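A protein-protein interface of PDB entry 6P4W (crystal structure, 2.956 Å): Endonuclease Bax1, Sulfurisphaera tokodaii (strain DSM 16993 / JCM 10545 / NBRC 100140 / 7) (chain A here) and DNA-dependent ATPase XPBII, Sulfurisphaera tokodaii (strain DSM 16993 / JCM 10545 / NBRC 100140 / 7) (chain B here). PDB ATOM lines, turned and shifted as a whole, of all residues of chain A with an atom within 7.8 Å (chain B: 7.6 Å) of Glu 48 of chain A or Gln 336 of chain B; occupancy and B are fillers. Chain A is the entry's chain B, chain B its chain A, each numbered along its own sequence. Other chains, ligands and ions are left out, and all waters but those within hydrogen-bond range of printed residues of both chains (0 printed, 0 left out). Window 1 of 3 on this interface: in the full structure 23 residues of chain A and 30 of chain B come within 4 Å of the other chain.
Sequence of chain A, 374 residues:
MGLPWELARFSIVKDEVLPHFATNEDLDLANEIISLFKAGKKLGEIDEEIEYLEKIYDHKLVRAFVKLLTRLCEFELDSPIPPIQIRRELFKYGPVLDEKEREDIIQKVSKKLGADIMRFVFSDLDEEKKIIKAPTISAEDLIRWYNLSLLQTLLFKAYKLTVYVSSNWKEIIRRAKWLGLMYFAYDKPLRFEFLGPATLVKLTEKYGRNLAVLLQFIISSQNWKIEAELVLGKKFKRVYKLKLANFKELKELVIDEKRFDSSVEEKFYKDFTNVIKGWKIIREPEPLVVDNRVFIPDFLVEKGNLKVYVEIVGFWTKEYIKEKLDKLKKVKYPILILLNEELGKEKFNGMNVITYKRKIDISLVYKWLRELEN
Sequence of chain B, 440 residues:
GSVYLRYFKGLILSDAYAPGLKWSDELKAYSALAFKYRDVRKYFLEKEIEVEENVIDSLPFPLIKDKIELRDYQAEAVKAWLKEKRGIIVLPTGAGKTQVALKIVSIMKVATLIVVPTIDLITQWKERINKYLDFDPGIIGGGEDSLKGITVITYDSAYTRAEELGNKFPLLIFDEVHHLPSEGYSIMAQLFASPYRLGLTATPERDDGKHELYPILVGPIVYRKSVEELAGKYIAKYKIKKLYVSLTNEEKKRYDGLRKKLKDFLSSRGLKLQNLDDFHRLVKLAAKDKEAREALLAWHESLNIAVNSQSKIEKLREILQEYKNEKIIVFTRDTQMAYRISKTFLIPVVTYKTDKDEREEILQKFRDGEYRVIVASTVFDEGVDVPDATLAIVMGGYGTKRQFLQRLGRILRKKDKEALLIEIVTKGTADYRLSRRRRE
OE2 of Glu 48 of chain A sits close to N of Gln 336 of chain B.
OE2 of Glu 128 of chain A sits at hydrogen-bond distance from NE2 of Gln 336 of chain B (3.0 Å).
OD1 of Asp 334 of chain B lies close to OE1 of Glu 48 of chain A, 3.1 Å away.
The side-chain hydroxyl (OH) of Tyr 339 of chain B lies close to the side-chain carboxylate (OE2) of Glu 127 of chain A, at 2.4 Å.
O of Asp 334 of chain B is in hydrogen-bond range of OG1 of Thr 332 of chain B, at 2.7 Å.
NE of Arg 333 of chain B is in salt-bridge range of OD2 of Asp 334 of chain B, at 3.5 Å.
The side-chain hydroxyl (OG1) of Thr 335 of chain B is in hydrogen-bond range of the side-chain amide oxygen (OE1) of Gln 336 of chain B (3.3 Å).
The side-chain carboxylate of Glu 45 of chain A sits at hydrogen-bond distance from the backbone NH of Lys 42 of chain A, at 3.1 Å.
The side-chain carboxylate (OE1) of Glu 128 of chain A is in salt-bridge range of the side-chain amino group (NZ) of Lys 42 of chain A, 2.8 Å away.
The backbone carbonyl oxygen of Glu 127 of chain A is in hydrogen-bond range of the backbone NH of Gly 44 of chain A, at 2.9 Å.
O of Gly 44 of chain A touches CG of Gln 336 of chain B (3.5 Å).
Glu 45 of chain A touches Gln 336 of chain B (N to CD, 3.997 Å).
Glu 48 of chain A touches Thr 335 of chain B (OE2 to N, 3.6 Å).
Tyr 52 of chain A touches Leu 297 of chain B.
CE1 of His 300 of chain B touches CB of Tyr 52 of chain A, 3.2 Å away.
Glu 127 of chain A touches Gln 336 of chain B (CB to OE1, 3.8 Å).
Glu 127 of chain A touches Thr 351 of chain B.
Glu 128 of chain A touches Tyr 339 of chain B.
Printed residues of chain B within 4 Å of Glu 48 of chain A: Asp 334 (3.1 Å), Thr 335 (3.6 Å) and Gln 336 (3.2 Å).
Of the printed residues of chain A, Gln 336 of chain B touches Gly 44 (3.5 Å), Glu 45 (3.997 Å), Glu 48 (3.2 Å), Glu 127 (3.8 Å) and Glu 128 (3.0 Å).
Printed residues of chain A within 4 Å of His 300 of chain B: Tyr 52 (3.2 Å).
Printed residues of chain A within 4 Å of Asp 334 of chain B: Glu 48 (3.1 Å).
Of the printed residues of chain B, Glu 45 of chain A touches Gln 336.
Of the printed residues of chain B, Tyr 52 of chain A touches Leu 297 (3.5 Å) and His 300 (3.2 Å).
Printed residues of chain A within 4 Å of Thr 335 of chain B: Glu 48 (3.6 Å).
The nearest residue of chain B that does not touch Glu 48 of chain A is Asn 304 of chain B (4.6 Å).
Of the 17 printed residues of chain A, 6 touch a printed residue of chain B.
Hydrophobic or aromatic side chains of chain A that line the printed part of chain B: Tyr 52.
Of the 17 printed residues of chain B, 7 touch a printed residue of chain A.
Printed residues of chain B that touch a printed residue of chain A: Leu 297, His 300, Asp 334, Thr 335, Gln 336, Tyr 339 and Thr 351.
Hydrophobic or aromatic side chains of chain B that line the printed part of chain A: Leu 297, His 300 and Tyr 339.
Among the printed residues, no Asp or Glu carboxylate lies within 4 Å of a Lys or Arg side-chain nitrogen of the other chain.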
ATOM      1  N   LEU A  36     -22.427   4.514 -31.067  1.00  0.00           N
ATOM      2  CA  LEU A  36     -23.055   3.287 -30.580  1.00  0.00           C
ATOM      3  C   LEU A  36     -23.994   3.529 -29.413  1.00  0.00           C
ATOM      4  O   LEU A  36     -24.836   2.672 -29.124  1.00  0.00           O
ATOM      5  CB  LEU A  36     -22.014   2.257 -30.144  1.00  0.00           C
ATOM      6  CG  LEU A  36     -21.173   1.866 -31.333  1.00  0.00           C
ATOM      7  CD1 LEU A  36     -20.286   0.753 -30.894  1.00  0.00           C
ATOM      8  CD2 LEU A  36     -22.102   1.478 -32.481  1.00  0.00           C
ATOM      9  N   LYS A  42     -29.256  -1.935 -25.733  1.00  0.00           N
ATOM     10  CA  LYS A  42     -28.798  -2.615 -24.528  1.00  0.00           C
ATOM     11  C   LYS A  42     -27.269  -2.575 -24.430  1.00  0.00           C
ATOM     12  O   LYS A  42     -26.560  -2.633 -25.438  1.00  0.00           O
ATOM     13  CB  LYS A  42     -29.298  -4.059 -24.503  1.00  0.00           C
ATOM     14  CG  LYS A  42     -30.816  -4.229 -24.527  1.00  0.00           C
ATOM     15  CD  LYS A  42     -31.157  -5.711 -24.577  1.00  0.00           C
ATOM     16  CE  LYS A  42     -32.639  -5.981 -24.702  1.00  0.00           C
ATOM     17  NZ  LYS A  42     -32.881  -7.463 -24.764  1.00  0.00           N
ATOM     18  N   LEU A  43     -26.761  -2.482 -23.198  1.00  0.00           N
ATOM     19  CA  LEU A  43     -25.316  -2.360 -23.012  1.00  0.00           C
ATOM     20  C   LEU A  43     -24.577  -3.571 -23.560  1.00  0.00           C
ATOM     21  O   LEU A  43     -23.439  -3.442 -24.028  1.00  0.00           O
ATOM     22  CB  LEU A  43     -24.986  -2.191 -21.530  1.00  0.00           C
ATOM     23  CG  LEU A  43     -25.472  -0.899 -20.878  1.00  0.00           C
ATOM     24  CD1 LEU A  43     -25.131  -0.853 -19.392  1.00  0.00           C
ATOM     25  CD2 LEU A  43     -24.907   0.292 -21.626  1.00  0.00           C
ATOM     26  N   GLY A  44     -25.214  -4.748 -23.519  1.00  0.00           N
ATOM     27  CA  GLY A  44     -24.625  -5.973 -24.035  1.00  0.00           C
ATOM     28  C   GLY A  44     -24.631  -6.083 -25.546  1.00  0.00           C
ATOM     29  O   GLY A  44     -23.837  -6.846 -26.103  1.00  0.00           O
ATOM     30  N   GLU A  45     -25.554  -5.385 -26.210  1.00  0.00           N
ATOM     31  CA  GLU A  45     -25.459  -5.181 -27.651  1.00  0.00           C
ATOM     32  C   GLU A  45     -24.235  -4.333 -27.984  1.00  0.00           C
ATOM     33  O   GLU A  45     -23.506  -4.609 -28.944  1.00  0.00           O
ATOM     34  CB  GLU A  45     -26.742  -4.515 -28.161  1.00  0.00           C
ATOM     35  CG  GLU A  45     -28.015  -5.330 -27.849  1.00  0.00           C
ATOM     36  CD  GLU A  45     -29.325  -4.589 -28.152  1.00  0.00           C
ATOM     37  OE1 GLU A  45     -29.280  -3.385 -28.508  1.00  0.00           O
ATOM     38  OE2 GLU A  45     -30.401  -5.222 -28.016  1.00  0.00           O
ATOM     39  N   ILE A  46     -23.971  -3.313 -27.171  1.00  0.00           N
ATOM     40  CA  ILE A  46     -22.820  -2.480 -27.455  1.00  0.00           C
ATOM     41  C   ILE A  46     -21.529  -3.238 -27.180  1.00  0.00           C
ATOM     42  O   ILE A  46     -20.528  -3.035 -27.877  1.00  0.00           O
ATOM     43  CB  ILE A  46     -22.918  -1.180 -26.653  1.00  0.00           C
ATOM     44  CG1 ILE A  46     -24.096  -0.363 -27.178  1.00  0.00           C
ATOM     45  CG2 ILE A  46     -21.648  -0.385 -26.789  1.00  0.00           C
ATOM     46  CD1 ILE A  46     -24.416   0.854 -26.338  1.00  0.00           C
ATOM     47  N   ASP A  47     -21.530  -4.149 -26.201  1.00  0.00           N
ATOM     48  CA  ASP A  47     -20.325  -4.930 -25.961  1.00  0.00           C
ATOM     49  C   ASP A  47     -19.964  -5.768 -27.170  1.00  0.00           C
ATOM     50  O   ASP A  47     -18.779  -5.989 -27.433  1.00  0.00           O
ATOM     51  CB  ASP A  47     -20.488  -5.832 -24.744  1.00  0.00           C
ATOM     52  CG  ASP A  47     -20.346  -5.074 -23.445  1.00  0.00           C
ATOM     53  OD1 ASP A  47     -19.804  -3.950 -23.480  1.00  0.00           O
ATOM     54  OD2 ASP A  47     -20.750  -5.603 -22.386  1.00  0.00           O
ATOM     55  N   GLU A  48     -20.952  -6.188 -27.950  1.00  0.00           N
ATOM     56  CA  GLU A  48     -20.654  -6.988 -29.127  1.00  0.00           C
ATOM     57  C   GLU A  48     -20.350  -6.123 -30.344  1.00  0.00           C
ATOM     58  O   GLU A  48     -19.637  -6.562 -31.253  1.00  0.00           O
ATOM     59  CB  GLU A  48     -21.814  -7.954 -29.407  1.00  0.00           C
ATOM     60  CG  GLU A  48     -22.038  -8.980 -28.276  1.00  0.00           C
ATOM     61  CD  GLU A  48     -23.284  -9.882 -28.454  1.00  0.00           C
ATOM     62  OE1 GLU A  48     -24.032  -9.718 -29.447  1.00  0.00           O
ATOM     63  OE2 GLU A  48     -23.535 -10.739 -27.569  1.00  0.00           O
ATOM     64  N   GLU A  49     -20.866  -4.905 -30.386  1.00  0.00           N
ATOM     65  CA  GLU A  49     -20.609  -4.033 -31.516  1.00  0.00           C
ATOM     66  C   GLU A  49     -19.226  -3.394 -31.519  1.00  0.00           C
ATOM     67  O   GLU A  49     -18.831  -2.867 -32.562  1.00  0.00           O
ATOM     68  CB  GLU A  49     -21.660  -2.933 -31.552  1.00  0.00           C
ATOM     69  CG  GLU A  49     -23.027  -3.366 -32.048  1.00  0.00           C
ATOM     70  CD  GLU A  49     -24.108  -2.312 -31.854  1.00  0.00           C
ATOM     71  OE1 GLU A  49     -23.909  -1.379 -31.047  1.00  0.00           O
ATOM     72  OE2 GLU A  49     -25.157  -2.414 -32.532  1.00  0.00           O
ATOM     73  N   ILE A  50     -18.472  -3.457 -30.419  1.00  0.00           N
ATOM     74  CA  ILE A  50     -17.182  -2.781 -30.288  1.00  0.00           C
ATOM     75  C   ILE A  50     -16.047  -3.757 -30.490  1.00  0.00           C
ATOM     76  O   ILE A  50     -14.865  -3.443 -30.269  1.00  0.00           O
ATOM     77  CB  ILE A  50     -17.057  -2.140 -28.905  1.00  0.00           C
ATOM     78  CG1 ILE A  50     -17.008  -3.212 -27.803  1.00  0.00           C
ATOM     79  CG2 ILE A  50     -18.199  -1.141 -28.689  1.00  0.00           C
ATOM     80  CD1 ILE A  50     -16.785  -2.668 -26.418  1.00  0.00           C
ATOM     81  N   GLU A  51     -16.423  -5.013 -30.656  1.00  0.00           N
ATOM     82  CA  GLU A  51     -15.485  -6.127 -30.633  1.00  0.00           C
ATOM     83  C   GLU A  51     -14.425  -6.036 -31.649  1.00  0.00           C
ATOM     84  O   GLU A  51     -13.296  -6.352 -31.401  1.00  0.00           O
ATOM     85  CB  GLU A  51     -16.238  -7.420 -30.845  1.00  0.00           C
ATOM     86  CG  GLU A  51     -16.552  -8.176 -29.574  1.00  0.00           C
ATOM     87  CD  GLU A  51     -17.498  -9.333 -29.812  1.00  0.00           C
ATOM     88  OE1 GLU A  51     -17.945  -9.507 -30.957  1.00  0.00           O
ATOM     89  OE2 GLU A  51     -17.808 -10.066 -28.854  1.00  0.00           O
ATOM     90  N   TYR A  52     -14.825  -5.668 -32.827  1.00  0.00           N
ATOM     91  CA  TYR A  52     -13.902  -5.368 -33.932  1.00  0.00           C
ATOM     92  C   TYR A  52     -13.081  -4.111 -33.636  1.00  0.00           C
ATOM     93  O   TYR A  52     -11.933  -3.992 -34.087  1.00  0.00           O
ATOM     94  CB  TYR A  52     -14.682  -5.207 -35.260  1.00  0.00           C
ATOM     95  CG  TYR A  52     -15.264  -3.819 -35.545  1.00  0.00           C
ATOM     96  CD1 TYR A  52     -16.278  -3.261 -34.749  1.00  0.00           C
ATOM     97  CD2 TYR A  52     -14.849  -3.102 -36.661  1.00  0.00           C
ATOM     98  CE1 TYR A  52     -16.807  -1.995 -35.056  1.00  0.00           C
ATOM     99  CE2 TYR A  52     -15.380  -1.850 -36.968  1.00  0.00           C
ATOM    100  CZ  TYR A  52     -16.355  -1.302 -36.160  1.00  0.00           C
ATOM    101  OH  TYR A  52     -16.920  -0.069 -36.416  1.00  0.00           O
ATOM    102  N   LEU A  53     -13.643  -3.159 -32.891  1.00  0.00           N
ATOM    103  CA  LEU A  53     -12.854  -1.992 -32.500  1.00  0.00           C
ATOM    104  C   LEU A  53     -11.738  -2.379 -31.546  1.00  0.00           C
ATOM    105  O   LEU A  53     -10.696  -1.713 -31.524  1.00  0.00           O
ATOM    106  CB  LEU A  53     -13.717  -0.926 -31.843  1.00  0.00           C
ATOM    107  CG  LEU A  53     -14.750  -0.296 -32.749  1.00  0.00           C
ATOM    108  CD1 LEU A  53     -15.601   0.645 -31.931  1.00  0.00           C
ATOM    109  CD2 LEU A  53     -14.059   0.431 -33.892  1.00  0.00           C
ATOM    110  N   ASP A 126     -26.288  -6.105 -16.123  1.00  0.00           N
ATOM    111  CA  ASP A 126     -25.742  -5.001 -16.910  1.00  0.00           C
ATOM    112  C   ASP A 126     -25.992  -5.216 -18.395  1.00  0.00           C
ATOM    113  O   ASP A 126     -26.473  -4.319 -19.093  1.00  0.00           O
ATOM    114  CB  ASP A 126     -24.238  -4.862 -16.653  1.00  0.00           C
ATOM    115  CG  ASP A 126     -23.908  -4.303 -15.271  1.00  0.00           C
ATOM    116  OD1 ASP A 126     -24.674  -3.453 -14.754  1.00  0.00           O
ATOM    117  OD2 ASP A 126     -22.860  -4.712 -14.710  1.00  0.00           O
ATOM    118  N   GLU A 127     -25.703  -6.424 -18.885  1.00  0.00           N
ATOM    119  CA  GLU A 127     -25.809  -6.692 -20.311  1.00  0.00           C
ATOM    120  C   GLU A 127     -27.184  -6.382 -20.877  1.00  0.00           C
ATOM    121  O   GLU A 127     -27.287  -6.113 -22.075  1.00  0.00           O
ATOM    122  CB  GLU A 127     -25.533  -8.161 -20.594  1.00  0.00           C
ATOM    123  CG  GLU A 127     -24.159  -8.651 -20.304  1.00  0.00           C
ATOM    124  CD  GLU A 127     -24.162  -9.722 -19.238  1.00  0.00           C
ATOM    125  OE1 GLU A 127     -23.079 -10.019 -18.713  1.00  0.00           O
ATOM    126  OE2 GLU A 127     -25.241 -10.251 -18.900  1.00  0.00           O
ATOM    127  N   GLU A 128     -28.235  -6.389 -20.056  1.00  0.00           N
ATOM    128  CA  GLU A 128     -29.596  -6.244 -20.559  1.00  0.00           C
ATOM    129  C   GLU A 128     -30.231  -4.891 -20.275  1.00  0.00           C
ATOM    130  O   GLU A 128     -31.343  -4.644 -20.753  1.00  0.00           O
ATOM    131  CB  GLU A 128     -30.482  -7.359 -19.993  1.00  0.00           C
ATOM    132  CG  GLU A 128     -30.186  -8.701 -20.618  1.00  0.00           C
ATOM    133  CD  GLU A 128     -30.623  -8.756 -22.069  1.00  0.00           C
ATOM    134  OE1 GLU A 128     -31.715  -8.238 -22.387  1.00  0.00           O
ATOM    135  OE2 GLU A 128     -29.861  -9.288 -22.900  1.00  0.00           O
ATOM    136  N   LYS A 129     -29.552  -4.004 -19.538  1.00  0.00           N
ATOM    137  CA  LYS A 129     -30.075  -2.664 -19.294  1.00  0.00           C
ATOM    138  C   LYS A 129     -30.196  -1.879 -20.595  1.00  0.00           C
ATOM    139  O   LYS A 129     -29.235  -1.757 -21.358  1.00  0.00           O
ATOM    140  CB  LYS A 129     -29.177  -1.926 -18.303  1.00  0.00           C
ATOM    141  CG  LYS A 129     -29.197  -2.547 -16.903  1.00  0.00           C
ATOM    142  CD  LYS A 129     -28.303  -1.820 -15.905  1.00  0.00           C
ATOM    143  CE  LYS A 129     -28.299  -2.509 -14.534  1.00  0.00           C
ATOM    144  NZ  LYS A 129     -29.582  -2.373 -13.761  1.00  0.00           N
ATOM    145  N   LEU B 297     -15.968  -4.117 -40.516  1.00  0.00           N
ATOM    146  CA  LEU B 297     -17.268  -4.150 -39.856  1.00  0.00           C
ATOM    147  C   LEU B 297     -18.236  -5.074 -40.591  1.00  0.00           C
ATOM    148  O   LEU B 297     -18.958  -5.858 -39.961  1.00  0.00           O
ATOM    149  CB  LEU B 297     -17.844  -2.741 -39.743  1.00  0.00           C
ATOM    150  CG  LEU B 297     -19.119  -2.750 -38.890  1.00  0.00           C
ATOM    151  CD1 LEU B 297     -18.892  -3.402 -37.523  1.00  0.00           C
ATOM    152  CD2 LEU B 297     -19.716  -1.366 -38.736  1.00  0.00           C
ATOM    153  N   HIS B 300     -17.479  -8.621 -39.735  1.00  0.00           N
ATOM    154  CA  HIS B 300     -18.018  -9.008 -38.430  1.00  0.00           C
ATOM    155  C   HIS B 300     -19.536  -9.113 -38.466  1.00  0.00           C
ATOM    156  O   HIS B 300     -20.109 -10.080 -37.957  1.00  0.00           O
ATOM    157  CB  HIS B 300     -17.588  -8.027 -37.343  1.00  0.00           C
ATOM    158  CG  HIS B 300     -16.171  -8.198 -36.909  1.00  0.00           C
ATOM    159  ND1 HIS B 300     -15.129  -7.527 -37.507  1.00  0.00           N
ATOM    160  CD2 HIS B 300     -15.619  -8.967 -35.946  1.00  0.00           C
ATOM    161  CE1 HIS B 300     -13.992  -7.881 -36.935  1.00  0.00           C
ATOM    162  NE2 HIS B 300     -14.263  -8.751 -35.980  1.00  0.00           N
ATOM    163  N   ASN B 304     -21.765 -12.413 -37.763  1.00  0.00           N
ATOM    164  CA  ASN B 304     -22.725 -12.410 -36.660  1.00  0.00           C
ATOM    165  C   ASN B 304     -24.103 -12.911 -37.115  1.00  0.00           C
ATOM    166  O   ASN B 304     -24.776 -13.638 -36.378  1.00  0.00           O
ATOM    167  CB  ASN B 304     -22.792 -10.986 -36.072  1.00  0.00           C
ATOM    168  CG  ASN B 304     -23.334 -10.933 -34.650  1.00  0.00           C
ATOM    169  OD1 ASN B 304     -24.006 -11.852 -34.188  1.00  0.00           O
ATOM    170  ND2 ASN B 304     -23.057  -9.837 -33.960  1.00  0.00           N
ATOM    171  N   ASN B 308     -25.731 -16.327 -35.517  1.00  0.00           N
ATOM    172  CA  ASN B 308     -26.808 -16.090 -34.562  1.00  0.00           C
ATOM    173  C   ASN B 308     -28.161 -15.969 -35.260  1.00  0.00           C
ATOM    174  O   ASN B 308     -29.007 -15.180 -34.851  1.00  0.00           O
ATOM    175  CB  ASN B 308     -26.498 -14.864 -33.687  1.00  0.00           C
ATOM    176  CG  ASN B 308     -25.257 -15.065 -32.795  1.00  0.00           C
ATOM    177  OD1 ASN B 308     -25.099 -16.098 -32.134  1.00  0.00           O
ATOM    178  ND2 ASN B 308     -24.388 -14.071 -32.773  1.00  0.00           N
ATOM    179  N   THR B 332     -23.788 -21.004 -26.222  1.00  0.00           N
ATOM    180  CA  THR B 332     -23.615 -19.960 -27.217  1.00  0.00           C
ATOM    181  C   THR B 332     -22.255 -19.337 -26.969  1.00  0.00           C
ATOM    182  O   THR B 332     -21.592 -19.654 -25.984  1.00  0.00           O
ATOM    183  CB  THR B 332     -24.719 -18.884 -27.165  1.00  0.00           C
ATOM    184  OG1 THR B 332     -24.579 -18.122 -25.968  1.00  0.00           O
ATOM    185  CG2 THR B 332     -26.125 -19.487 -27.208  1.00  0.00           C
ATOM    186  N   ARG B 333     -21.801 -18.500 -27.897  1.00  0.00           N
ATOM    187  CA  ARG B 333     -20.620 -17.710 -27.578  1.00  0.00           C
ATOM    188  C   ARG B 333     -21.029 -16.333 -27.066  1.00  0.00           C
ATOM    189  O   ARG B 333     -20.585 -15.913 -25.994  1.00  0.00           O
ATOM    190  CB  ARG B 333     -19.654 -17.629 -28.785  1.00  0.00           C
ATOM    191  CG  ARG B 333     -20.015 -16.714 -29.970  1.00  0.00           C
ATOM    192  CD  ARG B 333     -18.785 -16.310 -30.843  1.00  0.00           C
ATOM    193  NE  ARG B 333     -18.008 -15.177 -30.310  1.00  0.00           N
ATOM    194  CZ  ARG B 333     -16.978 -15.271 -29.457  1.00  0.00           C
ATOM    195  NH1 ARG B 333     -16.356 -14.170 -29.039  1.00  0.00           N
ATOM    196  NH2 ARG B 333     -16.554 -16.457 -29.022  1.00  0.00           N
ATOM    197  N   ASP B 334     -21.916 -15.655 -27.787  1.00  0.00           N
ATOM    198  CA  ASP B 334     -22.385 -14.344 -27.372  1.00  0.00           C
ATOM    199  C   ASP B 334     -23.309 -14.479 -26.167  1.00  0.00           C
ATOM    200  O   ASP B 334     -24.031 -15.465 -26.028  1.00  0.00           O
ATOM    201  CB  ASP B 334     -23.146 -13.664 -28.520  1.00  0.00           C
ATOM    202  CG  ASP B 334     -22.260 -13.300 -29.726  1.00  0.00           C
ATOM    203  OD1 ASP B 334     -22.564 -12.274 -30.376  1.00  0.00           O
ATOM    204  OD2 ASP B 334     -21.297 -14.024 -30.053  1.00  0.00           O
ATOM    205  N   THR B 335     -23.311 -13.463 -25.300  1.00  0.00           N
ATOM    206  CA  THR B 335     -24.268 -13.465 -24.195  1.00  0.00           C
ATOM    207  C   THR B 335     -25.673 -13.112 -24.674  1.00  0.00           C
ATOM    208  O   THR B 335     -26.663 -13.616 -24.134  1.00  0.00           O
ATOM    209  CB  THR B 335     -23.828 -12.507 -23.093  1.00  0.00           C
ATOM    210  OG1 THR B 335     -23.681 -11.187 -23.633  1.00  0.00           O
ATOM    211  CG2 THR B 335     -22.517 -12.959 -22.517  1.00  0.00           C
ATOM    212  N   GLN B 336     -25.776 -12.189 -25.633  1.00  0.00           N
ATOM    213  CA  GLN B 336     -27.081 -11.746 -26.101  1.00  0.00           C
ATOM    214  C   GLN B 336     -27.887 -12.903 -26.677  1.00  0.00           C
ATOM    215  O   GLN B 336     -29.109 -12.960 -26.503  1.00  0.00           O
ATOM    216  CB  GLN B 336     -26.910 -10.614 -27.111  1.00  0.00           C
ATOM    217  CG  GLN B 336     -26.281  -9.368 -26.503  1.00  0.00           C
ATOM    218  CD  GLN B 336     -26.919  -8.995 -25.169  1.00  0.00           C
ATOM    219  OE1 GLN B 336     -26.351  -9.232 -24.102  1.00  0.00           O
ATOM    220  NE2 GLN B 336     -28.111  -8.403 -25.231  1.00  0.00           N
ATOM    221  N   MET B 337     -27.231 -13.834 -27.373  1.00  0.00           N
ATOM    222  CA  MET B 337     -27.952 -15.001 -27.877  1.00  0.00           C
ATOM    223  C   MET B 337     -28.500 -15.843 -26.730  1.00  0.00           C
ATOM    224  O   MET B 337     -29.640 -16.313 -26.783  1.00  0.00           O
ATOM    225  CB  MET B 337     -27.050 -15.830 -28.789  1.00  0.00           C
ATOM    226  CG  MET B 337     -27.749 -16.945 -29.561  1.00  0.00           C
ATOM    227  SD  MET B 337     -28.817 -16.378 -30.902  1.00  0.00           S
ATOM    228  CE  MET B 337     -29.569 -17.908 -31.480  1.00  0.00           C
ATOM    229  N   ALA B 338     -27.714 -16.013 -25.669  1.00  0.00           N
ATOM    230  CA  ALA B 338     -28.181 -16.791 -24.530  1.00  0.00           C
ATOM    231  C   ALA B 338     -29.453 -16.207 -23.929  1.00  0.00           C
ATOM    232  O   ALA B 338     -30.307 -16.956 -23.438  1.00  0.00           O
ATOM    233  CB  ALA B 338     -27.081 -16.868 -23.471  1.00  0.00           C
ATOM    234  N   TYR B 339     -29.595 -14.881 -23.953  1.00  0.00           N
ATOM    235  CA  TYR B 339     -30.799 -14.254 -23.417  1.00  0.00           C
ATOM    236  C   TYR B 339     -31.979 -14.422 -24.368  1.00  0.00           C
ATOM    237  O   TYR B 339     -33.111 -14.642 -23.917  1.00  0.00           O
ATOM    238  CB  TYR B 339     -30.541 -12.770 -23.100  1.00  0.00           C
ATOM    239  CG  TYR B 339     -29.554 -12.553 -21.955  1.00  0.00           C
ATOM    240  CD1 TYR B 339     -29.806 -13.064 -20.676  1.00  0.00           C
ATOM    241  CD2 TYR B 339     -28.366 -11.861 -22.157  1.00  0.00           C
ATOM    242  CE1 TYR B 339     -28.905 -12.886 -19.645  1.00  0.00           C
ATOM    243  CE2 TYR B 339     -27.461 -11.679 -21.124  1.00  0.00           C
ATOM    244  CZ  TYR B 339     -27.735 -12.193 -19.872  1.00  0.00           C
ATOM    245  OH  TYR B 339     -26.832 -12.013 -18.846  1.00  0.00           O
ATOM    246  N   ARG B 340     -31.736 -14.326 -25.686  1.00  0.00           N
ATOM    247  CA  ARG B 340     -32.775 -14.664 -26.661  1.00  0.00           C
ATOM    248  C   ARG B 340     -33.314 -16.063 -26.412  1.00  0.00           C
ATOM    249  O   ARG B 340     -34.530 -16.282 -26.423  1.00  0.00           O
ATOM    250  CB  ARG B 340     -32.235 -14.560 -28.095  1.00  0.00           C
ATOM    251  CG  ARG B 340     -32.532 -13.244 -28.800  1.00  0.00           C
ATOM    252  CD  ARG B 340     -31.412 -12.828 -29.736  1.00  0.00           C
ATOM    253  NE  ARG B 340     -31.549 -13.496 -31.023  1.00  0.00           N
ATOM    254  CZ  ARG B 340     -30.700 -13.364 -32.037  1.00  0.00           C
ATOM    255  NH1 ARG B 340     -29.631 -12.583 -31.913  1.00  0.00           N
ATOM    256  NH2 ARG B 340     -30.927 -14.010 -33.178  1.00  0.00           N
ATOM    257  N   ILE B 341     -32.420 -17.013 -26.156  1.00  0.00           N
ATOM    258  CA  ILE B 341     -32.806 -18.414 -26.022  1.00  0.00           C
ATOM    259  C   ILE B 341     -33.547 -18.640 -24.709  1.00  0.00           C
ATOM    260  O   ILE B 341     -34.502 -19.426 -24.650  1.00  0.00           O
ATOM    261  CB  ILE B 341     -31.553 -19.305 -26.170  1.00  0.00           C
ATOM    262  CG1 ILE B 341     -31.152 -19.379 -27.654  1.00  0.00           C
ATOM    263  CG2 ILE B 341     -31.795 -20.681 -25.631  1.00  0.00           C
ATOM    264  CD1 ILE B 341     -29.816 -19.995 -27.939  1.00  0.00           C
ATOM    265  N   SER B 342     -33.136 -17.936 -23.644  1.00  0.00           N
ATOM    266  CA  SER B 342     -33.787 -18.075 -22.345  1.00  0.00           C
ATOM    267  C   SER B 342     -35.166 -17.425 -22.326  1.00  0.00           C
ATOM    268  O   SER B 342     -36.101 -17.953 -21.716  1.00  0.00           O
ATOM    269  CB  SER B 342     -32.918 -17.440 -21.265  1.00  0.00           C
ATOM    270  OG  SER B 342     -33.555 -17.518 -20.006  1.00  0.00           O
ATOM    271  N   THR B 351     -24.171 -16.816 -17.801  1.00  0.00           N
ATOM    272  CA  THR B 351     -23.069 -16.163 -18.507  1.00  0.00           C
ATOM    273  C   THR B 351     -21.865 -16.031 -17.573  1.00  0.00           C
ATOM    274  O   THR B 351     -21.871 -16.497 -16.433  1.00  0.00           O
ATOM    275  CB  THR B 351     -23.487 -14.794 -19.066  1.00  0.00           C
ATOM    276  OG1 THR B 351     -23.690 -13.860 -18.004  1.00  0.00           O
ATOM    277  CG2 THR B 351     -24.767 -14.906 -19.846  1.00  0.00           C
ATOM    278  N   SER B 377     -23.455 -19.175 -21.884  1.00  0.00           N
ATOM    279  CA  SER B 377     -22.483 -18.602 -22.789  1.00  0.00           C
ATOM    280  C   SER B 377     -21.070 -19.072 -22.428  1.00  0.00           C
ATOM    281  O   SER B 377     -20.794 -19.536 -21.315  1.00  0.00           O
ATOM    282  CB  SER B 377     -22.575 -17.082 -22.758  1.00  0.00           C
ATOM    283  OG  SER B 377     -21.653 -16.565 -21.810  1.00  0.00           O
